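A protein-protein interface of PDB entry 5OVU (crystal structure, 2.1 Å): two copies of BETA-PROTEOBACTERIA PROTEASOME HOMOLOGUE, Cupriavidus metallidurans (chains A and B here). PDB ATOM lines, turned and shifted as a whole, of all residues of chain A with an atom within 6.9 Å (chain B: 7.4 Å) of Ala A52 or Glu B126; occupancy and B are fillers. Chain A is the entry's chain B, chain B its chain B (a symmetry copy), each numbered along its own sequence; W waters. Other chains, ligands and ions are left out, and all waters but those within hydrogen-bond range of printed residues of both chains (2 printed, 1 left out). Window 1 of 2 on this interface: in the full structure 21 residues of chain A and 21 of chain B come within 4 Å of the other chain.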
ATOM      1  N   THR A  21     -12.808   4.742 -17.959  1.00  0.00           N
ATOM      2  CA  THR A  21     -12.353   6.099 -18.254  1.00  0.00           C
ATOM      3  C   THR A  21     -10.834   6.175 -18.343  1.00  0.00           C
ATOM      4  O   THR A  21     -10.125   5.392 -17.714  1.00  0.00           O
ATOM      5  CB  THR A  21     -12.797   7.095 -17.161  1.00  0.00           C
ATOM      6  OG1 THR A  21     -12.108   6.810 -15.937  1.00  0.00           O
ATOM      7  CG2 THR A  21     -14.292   7.014 -16.913  1.00  0.00           C
ATOM      8  N   PHE A  22     -10.352   7.118 -19.147  1.00  0.00           N
ATOM      9  CA  PHE A  22      -8.971   7.570 -19.078  1.00  0.00           C
ATOM     10  C   PHE A  22      -9.000   8.880 -18.297  1.00  0.00           C
ATOM     11  O   PHE A  22      -9.248   9.942 -18.866  1.00  0.00           O
ATOM     12  CB  PHE A  22      -8.387   7.801 -20.476  1.00  0.00           C
ATOM     13  CG  PHE A  22      -8.025   6.538 -21.211  1.00  0.00           C
ATOM     14  CD1 PHE A  22      -7.120   5.634 -20.668  1.00  0.00           C
ATOM     15  CD2 PHE A  22      -8.562   6.268 -22.463  1.00  0.00           C
ATOM     16  CE1 PHE A  22      -6.777   4.477 -21.349  1.00  0.00           C
ATOM     17  CE2 PHE A  22      -8.221   5.114 -23.151  1.00  0.00           C
ATOM     18  CZ  PHE A  22      -7.326   4.219 -22.593  1.00  0.00           C
ATOM     19  N   GLY A  49      -8.946  -0.485  -9.792  1.00  0.00           N
ATOM     20  CA  GLY A  49      -8.039   0.546 -10.299  1.00  0.00           C
ATOM     21  C   GLY A  49      -8.348   1.072 -11.691  1.00  0.00           C
ATOM     22  O   GLY A  49      -9.376   0.741 -12.289  1.00  0.00           O
ATOM     23  N   THR A  50      -7.428   1.888 -12.202  1.00  0.00           N
ATOM     24  CA  THR A  50      -7.609   2.609 -13.466  1.00  0.00           C
ATOM     25  C   THR A  50      -7.671   1.698 -14.699  1.00  0.00           C
ATOM     26  O   THR A  50      -6.988   0.672 -14.765  1.00  0.00           O
ATOM     27  CB  THR A  50      -6.486   3.653 -13.675  1.00  0.00           C
ATOM     28  OG1 THR A  50      -6.793   4.478 -14.804  1.00  0.00           O
ATOM     29  CG2 THR A  50      -5.129   2.980 -13.901  1.00  0.00           C
ATOM     30  N   THR A  51      -8.485   2.101 -15.677  1.00  0.00           N
ATOM     31  CA  THR A  51      -8.613   1.383 -16.951  1.00  0.00           C
ATOM     32  C   THR A  51      -7.275   1.248 -17.680  1.00  0.00           C
ATOM     33  O   THR A  51      -7.039   0.253 -18.370  1.00  0.00           O
ATOM     34  CB  THR A  51      -9.603   2.096 -17.901  1.00  0.00           C
ATOM     35  OG1 THR A  51     -10.858   2.273 -17.239  1.00  0.00           O
ATOM     36  CG2 THR A  51      -9.819   1.290 -19.182  1.00  0.00           C
ATOM     37  N   ALA A  52      -6.409   2.249 -17.519  1.00  0.00           N
ATOM     38  CA  ALA A  52      -5.102   2.267 -18.170  1.00  0.00           C
ATOM     39  C   ALA A  52      -4.241   1.030 -17.885  1.00  0.00           C
ATOM     40  O   ALA A  52      -3.407   0.669 -18.709  1.00  0.00           O
ATOM     41  CB  ALA A  52      -4.344   3.534 -17.790  1.00  0.00           C
ATOM     42  N   HIS A  53      -4.435   0.389 -16.732  1.00  0.00           N
ATOM     43  CA  HIS A  53      -3.649  -0.797 -16.366  1.00  0.00           C
ATOM     44  C   HIS A  53      -4.348  -2.147 -16.612  1.00  0.00           C
ATOM     45  O   HIS A  53      -3.823  -3.193 -16.229  1.00  0.00           O
ATOM     46  CB  HIS A  53      -3.201  -0.698 -14.902  1.00  0.00           C
ATOM     47  CG  HIS A  53      -2.259   0.433 -14.636  1.00  0.00           C
ATOM     48  ND1 HIS A  53      -2.098   0.989 -13.385  1.00  0.00           N
ATOM     49  CD2 HIS A  53      -1.437   1.122 -15.462  1.00  0.00           C
ATOM     50  CE1 HIS A  53      -1.208   1.963 -13.451  1.00  0.00           C
ATOM     51  NE2 HIS A  53      -0.793   2.065 -14.701  1.00  0.00           N
ATOM     52  N   PHE A  54      -5.510  -2.132 -17.261  1.00  0.00           N
ATOM     53  CA  PHE A  54      -6.254  -3.367 -17.548  1.00  0.00           C
ATOM     54  C   PHE A  54      -5.591  -4.294 -18.584  1.00  0.00           C
ATOM     55  O   PHE A  54      -5.561  -5.507 -18.378  1.00  0.00           O
ATOM     56  CB  PHE A  54      -7.684  -3.039 -18.007  1.00  0.00           C
ATOM     57  CG  PHE A  54      -8.613  -2.584 -16.904  1.00  0.00           C
ATOM     58  CD1 PHE A  54      -8.160  -2.324 -15.607  1.00  0.00           C
ATOM     59  CD2 PHE A  54      -9.959  -2.381 -17.183  1.00  0.00           C
ATOM     60  CE1 PHE A  54      -9.035  -1.904 -14.619  1.00  0.00           C
ATOM     61  CE2 PHE A  54     -10.834  -1.953 -16.198  1.00  0.00           C
ATOM     62  CZ  PHE A  54     -10.372  -1.714 -14.914  1.00  0.00           C
ATOM     63  N   PRO A  55      -5.077  -3.740 -19.703  1.00  0.00           N
ATOM     64  CA  PRO A  55      -4.595  -4.614 -20.787  1.00  0.00           C
ATOM     65  C   PRO A  55      -3.506  -5.618 -20.393  1.00  0.00           C
ATOM     66  O   PRO A  55      -3.576  -6.782 -20.792  1.00  0.00           O
ATOM     67  CB  PRO A  55      -4.072  -3.622 -21.831  1.00  0.00           C
ATOM     68  CG  PRO A  55      -4.861  -2.385 -21.594  1.00  0.00           C
ATOM     69  CD  PRO A  55      -5.046  -2.320 -20.105  1.00  0.00           C
ATOM     70  N   VAL A  56      -2.509  -5.177 -19.634  1.00  0.00           N
ATOM     71  CA  VAL A  56      -1.440  -6.077 -19.194  1.00  0.00           C
ATOM     72  C   VAL A  56      -1.992  -7.163 -18.261  1.00  0.00           C
ATOM     73  O   VAL A  56      -1.661  -8.338 -18.417  1.00  0.00           O
ATOM     74  CB  VAL A  56      -0.276  -5.304 -18.523  1.00  0.00           C
ATOM     75  CG1 VAL A  56       0.649  -6.240 -17.750  1.00  0.00           C
ATOM     76  CG2 VAL A  56       0.512  -4.531 -19.571  1.00  0.00           C
ATOM     77  N   MET A  57      -2.836  -6.768 -17.310  1.00  0.00           N
ATOM     78  CA  MET A  57      -3.436  -7.715 -16.364  1.00  0.00           C
ATOM     79  C   MET A  57      -4.316  -8.762 -17.051  1.00  0.00           C
ATOM     80  O   MET A  57      -4.262  -9.942 -16.699  1.00  0.00           O
ATOM     81  CB  MET A  57      -4.246  -6.979 -15.287  1.00  0.00           C
ATOM     82  CG  MET A  57      -3.399  -6.344 -14.195  1.00  0.00           C
ATOM     83  SD  MET A  57      -2.425  -7.540 -13.258  1.00  0.00           S
ATOM     84  CE  MET A  57      -3.703  -8.456 -12.396  1.00  0.00           C
ATOM     85  N   LEU A  87       4.982  -9.676 -13.833  1.00  0.00           N
ATOM     86  CA  LEU A  87       4.891  -8.229 -14.058  1.00  0.00           C
ATOM     87  C   LEU A  87       6.267  -7.564 -14.072  1.00  0.00           C
ATOM     88  O   LEU A  87       6.535  -6.711 -14.919  1.00  0.00           O
ATOM     89  CB  LEU A  87       4.012  -7.560 -12.997  1.00  0.00           C
ATOM     90  CG  LEU A  87       2.497  -7.722 -13.130  1.00  0.00           C
ATOM     91  CD1 LEU A  87       1.812  -7.177 -11.885  1.00  0.00           C
ATOM     92  CD2 LEU A  87       1.970  -7.032 -14.380  1.00  0.00           C
ATOM     93  N   ILE A  93       7.076  -4.005 -14.788  1.00  0.00           N
ATOM     94  CA  ILE A  93       6.163  -3.213 -13.955  1.00  0.00           C
ATOM     95  C   ILE A  93       6.440  -3.512 -12.486  1.00  0.00           C
ATOM     96  O   ILE A  93       6.642  -4.668 -12.115  1.00  0.00           O
ATOM     97  CB  ILE A  93       4.685  -3.532 -14.280  1.00  0.00           C
ATOM     98  CG1 ILE A  93       4.328  -3.009 -15.677  1.00  0.00           C
ATOM     99  CG2 ILE A  93       3.746  -2.930 -13.238  1.00  0.00           C
ATOM    100  CD1 ILE A  93       3.036  -3.558 -16.242  1.00  0.00           C
ATOM    101  N   ARG B  73      -2.890  -5.605 -32.045  1.00  0.00           N
ATOM    102  CA  ARG B  73      -2.739  -5.150 -30.660  1.00  0.00           C
ATOM    103  C   ARG B  73      -1.547  -5.830 -29.975  1.00  0.00           C
ATOM    104  O   ARG B  73      -0.750  -5.172 -29.303  1.00  0.00           O
ATOM    105  CB  ARG B  73      -4.028  -5.415 -29.865  1.00  0.00           C
ATOM    106  CG  ARG B  73      -4.235  -4.494 -28.670  1.00  0.00           C
ATOM    107  CD  ARG B  73      -5.104  -5.147 -27.602  1.00  0.00           C
ATOM    108  NE  ARG B  73      -4.393  -6.232 -26.924  1.00  0.00           N
ATOM    109  CZ  ARG B  73      -3.496  -6.077 -25.945  1.00  0.00           C
ATOM    110  NH1 ARG B  73      -3.174  -4.868 -25.485  1.00  0.00           N
ATOM    111  NH2 ARG B  73      -2.908  -7.149 -25.417  1.00  0.00           N
ATOM    112  N   VAL B  76       1.813  -4.513 -31.591  1.00  0.00           N
ATOM    113  CA  VAL B  76       2.110  -3.179 -31.072  1.00  0.00           C
ATOM    114  C   VAL B  76       2.637  -3.305 -29.643  1.00  0.00           C
ATOM    115  O   VAL B  76       3.611  -2.649 -29.272  1.00  0.00           O
ATOM    116  CB  VAL B  76       0.869  -2.254 -31.105  1.00  0.00           C
ATOM    117  CG1 VAL B  76       1.142  -0.944 -30.378  1.00  0.00           C
ATOM    118  CG2 VAL B  76       0.441  -1.969 -32.540  1.00  0.00           C
ATOM    119  N   PHE B  77       1.992  -4.163 -28.858  1.00  0.00           N
ATOM    120  CA  PHE B  77       2.400  -4.418 -27.479  1.00  0.00           C
ATOM    121  C   PHE B  77       3.843  -4.925 -27.379  1.00  0.00           C
ATOM    122  O   PHE B  77       4.656  -4.347 -26.651  1.00  0.00           O
ATOM    123  CB  PHE B  77       1.421  -5.397 -26.812  1.00  0.00           C
ATOM    124  CG  PHE B  77       1.917  -5.962 -25.518  1.00  0.00           C
ATOM    125  CD1 PHE B  77       2.333  -5.119 -24.496  1.00  0.00           C
ATOM    126  CD2 PHE B  77       1.970  -7.338 -25.317  1.00  0.00           C
ATOM    127  CE1 PHE B  77       2.797  -5.632 -23.301  1.00  0.00           C
ATOM    128  CE2 PHE B  77       2.431  -7.858 -24.120  1.00  0.00           C
ATOM    129  CZ  PHE B  77       2.846  -7.000 -23.113  1.00  0.00           C
ATOM    130  N   PHE B  80       6.506  -2.208 -28.541  1.00  0.00           N
ATOM    131  CA  PHE B  80       6.781  -1.123 -27.600  1.00  0.00           C
ATOM    132  C   PHE B  80       7.426  -1.588 -26.289  1.00  0.00           C
ATOM    133  O   PHE B  80       8.071  -0.790 -25.612  1.00  0.00           O
ATOM    134  CB  PHE B  80       5.531  -0.265 -27.362  1.00  0.00           C
ATOM    135  CG  PHE B  80       5.353   0.818 -28.394  1.00  0.00           C
ATOM    136  CD1 PHE B  80       4.747   0.544 -29.614  1.00  0.00           C
ATOM    137  CD2 PHE B  80       5.835   2.099 -28.162  1.00  0.00           C
ATOM    138  CE1 PHE B  80       4.600   1.532 -30.573  1.00  0.00           C
ATOM    139  CE2 PHE B  80       5.692   3.093 -29.115  1.00  0.00           C
ATOM    140  CZ  PHE B  80       5.072   2.810 -30.324  1.00  0.00           C
ATOM    141  N   LEU B  81       7.279  -2.866 -25.942  1.00  0.00           N
ATOM    142  CA  LEU B  81       8.110  -3.466 -24.889  1.00  0.00           C
ATOM    143  C   LEU B  81       9.581  -3.396 -25.294  1.00  0.00           C
ATOM    144  O   LEU B  81      10.455  -3.142 -24.459  1.00  0.00           O
ATOM    145  CB  LEU B  81       7.731  -4.931 -24.630  1.00  0.00           C
ATOM    146  CG  LEU B  81       6.518  -5.251 -23.754  1.00  0.00           C
ATOM    147  CD1 LEU B  81       6.306  -6.760 -23.714  1.00  0.00           C
ATOM    148  CD2 LEU B  81       6.685  -4.700 -22.342  1.00  0.00           C
ATOM    149  N   GLU B  97       6.985   1.989 -14.758  1.00  0.00           N
ATOM    150  CA  GLU B  97       5.559   1.918 -14.438  1.00  0.00           C
ATOM    151  C   GLU B  97       5.356   1.228 -13.093  1.00  0.00           C
ATOM    152  O   GLU B  97       5.893   0.146 -12.853  1.00  0.00           O
ATOM    153  CB  GLU B  97       4.758   1.179 -15.517  1.00  0.00           C
ATOM    154  CG  GLU B  97       3.264   1.123 -15.202  1.00  0.00           C
ATOM    155  CD  GLU B  97       2.436   0.388 -16.242  1.00  0.00           C
ATOM    156  OE1 GLU B  97       2.790   0.414 -17.436  1.00  0.00           O
ATOM    157  OE2 GLU B  97       1.407  -0.206 -15.856  1.00  0.00           O
ATOM    158  N   GLU B  99       2.159  -0.155 -10.712  1.00  0.00           N
ATOM    159  CA  GLU B  99       0.757  -0.547 -10.836  1.00  0.00           C
ATOM    160  C   GLU B  99      -0.177   0.308  -9.974  1.00  0.00           C
ATOM    161  O   GLU B  99      -1.314   0.573 -10.364  1.00  0.00           O
ATOM    162  CB  GLU B  99       0.598  -2.025 -10.467  1.00  0.00           C
ATOM    163  CG  GLU B  99      -0.730  -2.644 -10.881  1.00  0.00           C
ATOM    164  CD  GLU B  99      -0.856  -2.887 -12.378  1.00  0.00           C
ATOM    165  OE1 GLU B  99       0.113  -2.644 -13.128  1.00  0.00           O
ATOM    166  OE2 GLU B  99      -1.939  -3.332 -12.805  1.00  0.00           O
ATOM    167  N   ASP B 101       0.023   3.457  -9.309  1.00  0.00           N
ATOM    168  CA  ASP B 101      -0.123   4.828  -9.807  1.00  0.00           C
ATOM    169  C   ASP B 101      -1.476   5.028 -10.484  1.00  0.00           C
ATOM    170  O   ASP B 101      -1.980   4.117 -11.140  1.00  0.00           O
ATOM    171  CB  ASP B 101       0.993   5.179 -10.801  1.00  0.00           C
ATOM    172  CG  ASP B 101       2.347   5.368 -10.132  1.00  0.00           C
ATOM    173  OD1 ASP B 101       2.412   5.423  -8.888  1.00  0.00           O
ATOM    174  OD2 ASP B 101       3.356   5.473 -10.858  1.00  0.00           O
ATOM    175  N   PRO B 102      -2.072   6.224 -10.323  1.00  0.00           N
ATOM    176  CA  PRO B 102      -3.315   6.526 -11.026  1.00  0.00           C
ATOM    177  C   PRO B 102      -3.040   6.939 -12.466  1.00  0.00           C
ATOM    178  O   PRO B 102      -1.885   6.957 -12.897  1.00  0.00           O
ATOM    179  CB  PRO B 102      -3.888   7.696 -10.224  1.00  0.00           C
ATOM    180  CG  PRO B 102      -2.691   8.399  -9.690  1.00  0.00           C
ATOM    181  CD  PRO B 102      -1.629   7.351  -9.480  1.00  0.00           C
ATOM    182  N   TYR B 103      -4.097   7.267 -13.203  1.00  0.00           N
ATOM    183  CA  TYR B 103      -3.957   7.728 -14.579  1.00  0.00           C
ATOM    184  C   TYR B 103      -3.190   9.052 -14.627  1.00  0.00           C
ATOM    185  O   TYR B 103      -3.485   9.974 -13.862  1.00  0.00           O
ATOM    186  CB  TYR B 103      -5.334   7.894 -15.224  1.00  0.00           C
ATOM    187  CG  TYR B 103      -5.287   8.431 -16.637  1.00  0.00           C
ATOM    188  CD1 TYR B 103      -5.015   7.590 -17.709  1.00  0.00           C
ATOM    189  CD2 TYR B 103      -5.520   9.781 -16.902  1.00  0.00           C
ATOM    190  CE1 TYR B 103      -4.972   8.073 -19.004  1.00  0.00           C
ATOM    191  CE2 TYR B 103      -5.481  10.275 -18.195  1.00  0.00           C
ATOM    192  CZ  TYR B 103      -5.204   9.416 -19.242  1.00  0.00           C
ATOM    193  OH  TYR B 103      -5.167   9.891 -20.529  1.00  0.00           O
ATOM    194  N   GLU B 104      -2.200   9.129 -15.518  1.00  0.00           N
ATOM    195  CA  GLU B 104      -1.407  10.347 -15.714  1.00  0.00           C
ATOM    196  C   GLU B 104      -1.190  10.607 -17.202  1.00  0.00           C
ATOM    197  O   GLU B 104      -0.801   9.706 -17.941  1.00  0.00           O
ATOM    198  CB  GLU B 104      -0.052  10.225 -15.012  1.00  0.00           C
ATOM    199  CG  GLU B 104      -0.147   9.775 -13.562  1.00  0.00           C
ATOM    200  CD  GLU B 104       1.114  10.050 -12.758  1.00  0.00           C
ATOM    201  OE1 GLU B 104       1.898  10.948 -13.142  1.00  0.00           O
ATOM    202  OE2 GLU B 104       1.320   9.366 -11.731  1.00  0.00           O
ATOM    203  N   GLN B 107       2.153   9.803 -19.074  1.00  0.00           N
ATOM    204  CA  GLN B 107       2.457   8.407 -19.418  1.00  0.00           C
ATOM    205  C   GLN B 107       1.988   8.000 -20.827  1.00  0.00           C
ATOM    206  O   GLN B 107       2.310   6.909 -21.297  1.00  0.00           O
ATOM    207  CB  GLN B 107       1.836   7.466 -18.380  1.00  0.00           C
ATOM    208  CG  GLN B 107       2.439   7.588 -16.991  1.00  0.00           C
ATOM    209  CD  GLN B 107       3.859   7.061 -16.923  1.00  0.00           C
ATOM    210  OE1 GLN B 107       4.125   5.916 -17.291  1.00  0.00           O
ATOM    211  NE2 GLN B 107       4.777   7.891 -16.447  1.00  0.00           N
ATOM    212  N   VAL B 109       2.106   7.640 -24.657  1.00  0.00           N
ATOM    213  CA  VAL B 109       3.226   7.571 -25.594  1.00  0.00           C
ATOM    214  C   VAL B 109       2.816   8.055 -26.983  1.00  0.00           C
ATOM    215  O   VAL B 109       3.412   8.990 -27.514  1.00  0.00           O
ATOM    216  CB  VAL B 109       3.794   6.143 -25.691  1.00  0.00           C
ATOM    217  CG1 VAL B 109       4.954   6.095 -26.682  1.00  0.00           C
ATOM    218  CG2 VAL B 109       4.241   5.667 -24.318  1.00  0.00           C
ATOM    219  N   GLY B 120      -3.687   3.021 -29.400  1.00  0.00           N
ATOM    220  CA  GLY B 120      -3.059   3.938 -28.453  1.00  0.00           C
ATOM    221  C   GLY B 120      -2.158   3.180 -27.489  1.00  0.00           C
ATOM    222  O   GLY B 120      -2.477   2.063 -27.091  1.00  0.00           O
ATOM    223  N   VAL B 121      -1.033   3.792 -27.113  1.00  0.00           N
ATOM    224  CA  VAL B 121      -0.050   3.160 -26.232  1.00  0.00           C
ATOM    225  C   VAL B 121       0.154   4.007 -24.975  1.00  0.00           C
ATOM    226  O   VAL B 121       0.423   5.204 -25.064  1.00  0.00           O
ATOM    227  CB  VAL B 121       1.302   2.962 -26.950  1.00  0.00           C
ATOM    228  CG1 VAL B 121       2.308   2.265 -26.037  1.00  0.00           C
ATOM    229  CG2 VAL B 121       1.112   2.172 -28.240  1.00  0.00           C
ATOM    230  N   TYR B 122       0.024   3.372 -23.810  1.00  0.00           N
ATOM    231  CA  TYR B 122       0.170   4.045 -22.519  1.00  0.00           C
ATOM    232  C   TYR B 122       1.311   3.408 -21.738  1.00  0.00           C
ATOM    233  O   TYR B 122       1.289   2.205 -21.472  1.00  0.00           O
ATOM    234  CB  TYR B 122      -1.130   3.934 -21.723  1.00  0.00           C
ATOM    235  CG  TYR B 122      -1.127   4.630 -20.376  1.00  0.00           C
ATOM    236  CD1 TYR B 122      -0.675   3.977 -19.231  1.00  0.00           C
ATOM    237  CD2 TYR B 122      -1.608   5.930 -20.240  1.00  0.00           C
ATOM    238  CE1 TYR B 122      -0.684   4.605 -17.993  1.00  0.00           C
ATOM    239  CE2 TYR B 122      -1.623   6.566 -19.007  1.00  0.00           C
ATOM    240  CZ  TYR B 122      -1.163   5.899 -17.886  1.00  0.00           C
ATOM    241  OH  TYR B 122      -1.175   6.529 -16.662  1.00  0.00           O
ATOM    242  N   SER B 123       2.310   4.219 -21.390  1.00  0.00           N
ATOM    243  CA  SER B 123       3.438   3.784 -20.559  1.00  0.00           C
ATOM    244  C   SER B 123       4.269   2.656 -21.197  1.00  0.00           C
ATOM    245  O   SER B 123       4.865   1.846 -20.488  1.00  0.00           O
ATOM    246  CB  SER B 123       2.931   3.365 -19.173  1.00  0.00           C
ATOM    247  OG  SER B 123       3.970   3.402 -18.215  1.00  0.00           O
ATOM    248  N   TYR B 124       4.289   2.607 -22.532  1.00  0.00           N
ATOM    249  CA  TYR B 124       5.085   1.638 -23.306  1.00  0.00           C
ATOM    250  C   TYR B 124       4.688   0.169 -23.107  1.00  0.00           C
ATOM    251  O   TYR B 124       5.392  -0.731 -23.571  1.00  0.00           O
ATOM    252  CB  TYR B 124       6.583   1.826 -23.022  1.00  0.00           C
ATOM    253  CG  TYR B 124       7.106   3.170 -23.463  1.00  0.00           C
ATOM    254  CD1 TYR B 124       7.017   4.284 -22.633  1.00  0.00           C
ATOM    255  CD2 TYR B 124       7.673   3.331 -24.723  1.00  0.00           C
ATOM    256  CE1 TYR B 124       7.492   5.521 -23.043  1.00  0.00           C
ATOM    257  CE2 TYR B 124       8.150   4.560 -25.144  1.00  0.00           C
ATOM    258  CZ  TYR B 124       8.056   5.653 -24.305  1.00  0.00           C
ATOM    259  OH  TYR B 124       8.532   6.866 -24.733  1.00  0.00           O
ATOM    260  N   ARG B 125       3.561  -0.072 -22.440  1.00  0.00           N
ATOM    261  CA  ARG B 125       3.191  -1.420 -22.001  1.00  0.00           C
ATOM    262  C   ARG B 125       1.704  -1.741 -22.191  1.00  0.00           C
ATOM    263  O   ARG B 125       1.356  -2.879 -22.503  1.00  0.00           O
ATOM    264  CB  ARG B 125       3.557  -1.603 -20.525  1.00  0.00           C
ATOM    265  CG  ARG B 125       5.040  -1.466 -20.192  1.00  0.00           C
ATOM    266  CD  ARG B 125       5.218  -1.265 -18.695  1.00  0.00           C
ATOM    267  NE  ARG B 125       6.615  -1.229 -18.255  1.00  0.00           N
ATOM    268  CZ  ARG B 125       7.390  -0.145 -18.226  1.00  0.00           C
ATOM    269  NH1 ARG B 125       6.946   1.040 -18.636  1.00  0.00           N
ATOM    270  NH2 ARG B 125       8.637  -0.246 -17.784  1.00  0.00           N
ATOM    271  N   GLU B 126       0.839  -0.747 -21.986  1.00  0.00           N
ATOM    272  CA  GLU B 126      -0.609  -0.927 -22.047  1.00  0.00           C
ATOM    273  C   GLU B 126      -1.129  -0.428 -23.400  1.00  0.00           C
ATOM    274  O   GLU B 126      -1.100   0.775 -23.676  1.00  0.00           O
ATOM    275  CB  GLU B 126      -1.289  -0.151 -20.911  1.00  0.00           C
ATOM    276  CG  GLU B 126      -0.586  -0.217 -19.555  1.00  0.00           C
ATOM    277  CD  GLU B 126      -0.815  -1.513 -18.801  1.00  0.00           C
ATOM    278  OE1 GLU B 126      -1.737  -2.283 -19.152  1.00  0.00           O
ATOM    279  OE2 GLU B 126      -0.066  -1.753 -17.832  1.00  0.00           O
ATOM    280  N   VAL B 127      -1.601  -1.351 -24.238  1.00  0.00           N
ATOM    281  CA  VAL B 127      -2.037  -1.017 -25.596  1.00  0.00           C
ATOM    282  C   VAL B 127      -3.546  -1.187 -25.765  1.00  0.00           C
ATOM    283  O   VAL B 127      -4.106  -2.218 -25.394  1.00  0.00           O
ATOM    284  CB  VAL B 127      -1.309  -1.883 -26.645  1.00  0.00           C
ATOM    285  CG1 VAL B 127      -1.693  -1.456 -28.060  1.00  0.00           C
ATOM    286  CG2 VAL B 127       0.198  -1.793 -26.444  1.00  0.00           C
ATOM    287  N   PHE B 128      -4.181  -0.167 -26.342  1.00  0.00           N
ATOM    288  CA  PHE B 128      -5.621  -0.158 -26.603  1.00  0.00           C
ATOM    289  C   PHE B 128      -5.916  -0.110 -28.099  1.00  0.00           C
ATOM    290  O   PHE B 128      -5.146   0.453 -28.877  1.00  0.00           O
ATOM    291  CB  PHE B 128      -6.270   1.057 -25.930  1.00  0.00           C
ATOM    292  CG  PHE B 128      -6.166   1.044 -24.435  1.00  0.00           C
ATOM    293  CD1 PHE B 128      -5.059   1.588 -23.795  1.00  0.00           C
ATOM    294  CD2 PHE B 128      -7.170   0.473 -23.666  1.00  0.00           C
ATOM    295  CE1 PHE B 128      -4.957   1.565 -22.413  1.00  0.00           C
ATOM    296  CE2 PHE B 128      -7.075   0.447 -22.284  1.00  0.00           C
ATOM    297  CZ  PHE B 128      -5.970   0.996 -21.656  1.00  0.00           C
HETATM  298  O   HOH W   1      -3.904  -0.560 -11.403  1.00  0.00           O
HETATM  299  O   HOH W   2      -0.329   5.138 -14.407  1.00  0.00           O
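No position is printed for both chains.
Of the 22 pairs that touch across the chains among the printed residues, none has its exchanged pair printed and touching as well.
A ring nitrogen (NE2) of His A53 sits close to the side-chain carboxylate (OE2) of Glu B97 (3.4 Å).
The backbone carbonyl oxygen of Glu B99 lies within hydrogen-bond range of a ring nitrogen (ND1) of His A53.
The side-chain carboxylate (OE1) of Glu B126 is in hydrogen-bond range of the backbone NH (N) of Val A56.
The backbone carbonyl oxygen of Ala A52 lies close to the side-chain carboxylate of Glu B126 (3.4 Å).
The guanidinium group (NH1) of Arg B125 sits at hydrogen-bond distance from the backbone carbonyl oxygen (O) of Ser B123, 2.9 Å away.
The backbone NH (N) of Phe B128 sits at hydrogen-bond distance from the backbone carbonyl oxygen (O) of Gly B120 (2.9 Å).
N of Glu B104 is in hydrogen-bond range of OH of Tyr B122 (3.0 Å).
The backbone NH of Thr A21 is in hydrogen-bond range of the side-chain hydroxyl of Thr A51 (3.2 Å).
The guanidinium group (NH1) of Arg B73 is in hydrogen-bond range of the backbone carbonyl oxygen (O) of Val B127 (2.8 Å).
The backbone carbonyl oxygen (O) of Leu A87 lies within hydrogen-bond range of the backbone NH (N) of Ile A93 (2.8 Å).
Of chain B, only Tyr B122, Glu B126 and Phe B128 come within 4 Å of Ala A52.
Of the printed residues of chain B, His A53 touches Glu B97, Glu B99, Asp B101 and Glu B126.
Printed residues of chain B within 4 Å of Pro A55: Arg B73 (3.96 Å), Glu B126 (3.4 Å), Val B127 (3.8 Å) and Phe B128 (3.6 Å).
Printed residues of chain B within 4 Å of Val A56: Arg B125 (3.5 Å) and Glu B126 (3.0 Å).
Of the printed residues of chain A, Asp B101 touches His A53.
Tyr B124 touches none of the printed residues of chain A.
Printed residues of chain A within 4 Å of Arg B125: Val A56 (3.5 Å) and Ile A93 (3.6 Å).
Glu B126 touches just these residues of chain A: Ala A52 (3.1 Å), His A53 (3.6 Å), Pro A55 (3.4 Å), Val A56 (3.0 Å) and Ile A93 (3.9 Å).
The nearest residue of chain B that does not touch Ala A52 is Tyr B103 (4.1 Å).
The nearest residue of chain A that does not touch Glu B126 is Phe A54 (4.2 Å).
Water W2 lies within hydrogen-bond range of the side-chain hydroxyl of Tyr B122 (2.8 Å), the backbone carbonyl oxygen of Pro B102 (2.8 Å) and a ring nitrogen (NE2) of His A53 (3.1 Å).
Water W1 bridges O of Glu B99 (3.0 Å) and ND1 of His A53 (3.1 Å).
Among the printed residues, pairs that only touch across the chains: His A53 with Asp B101, Pro A55 with Glu B126, Val A56 with Arg B125, Thr A51 with Phe B128, Ile A93 with Glu B97, Pro A55 with Phe B128, Phe A22 with Phe B128, Ile A93 with Arg B125, Met A57 with Glu B99, His A53 with Glu B126, Ile A93 with Glu B99, Phe A22 with Tyr B103, Thr A50 with Tyr B103, Ala A52 with Phe B128, Ala A52 with Tyr B122, Pro A55 with Val B127, Ile A93 with Glu B126 and Pro A55 with Arg B73.
Of the 13 printed residues of chain A, 9 touch a printed residue of chain B.
Along chain A the printed residues that touch a printed residue of chain B span positions 22 to 93.
Among the printed residues, 22 pairs touch across the chains.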
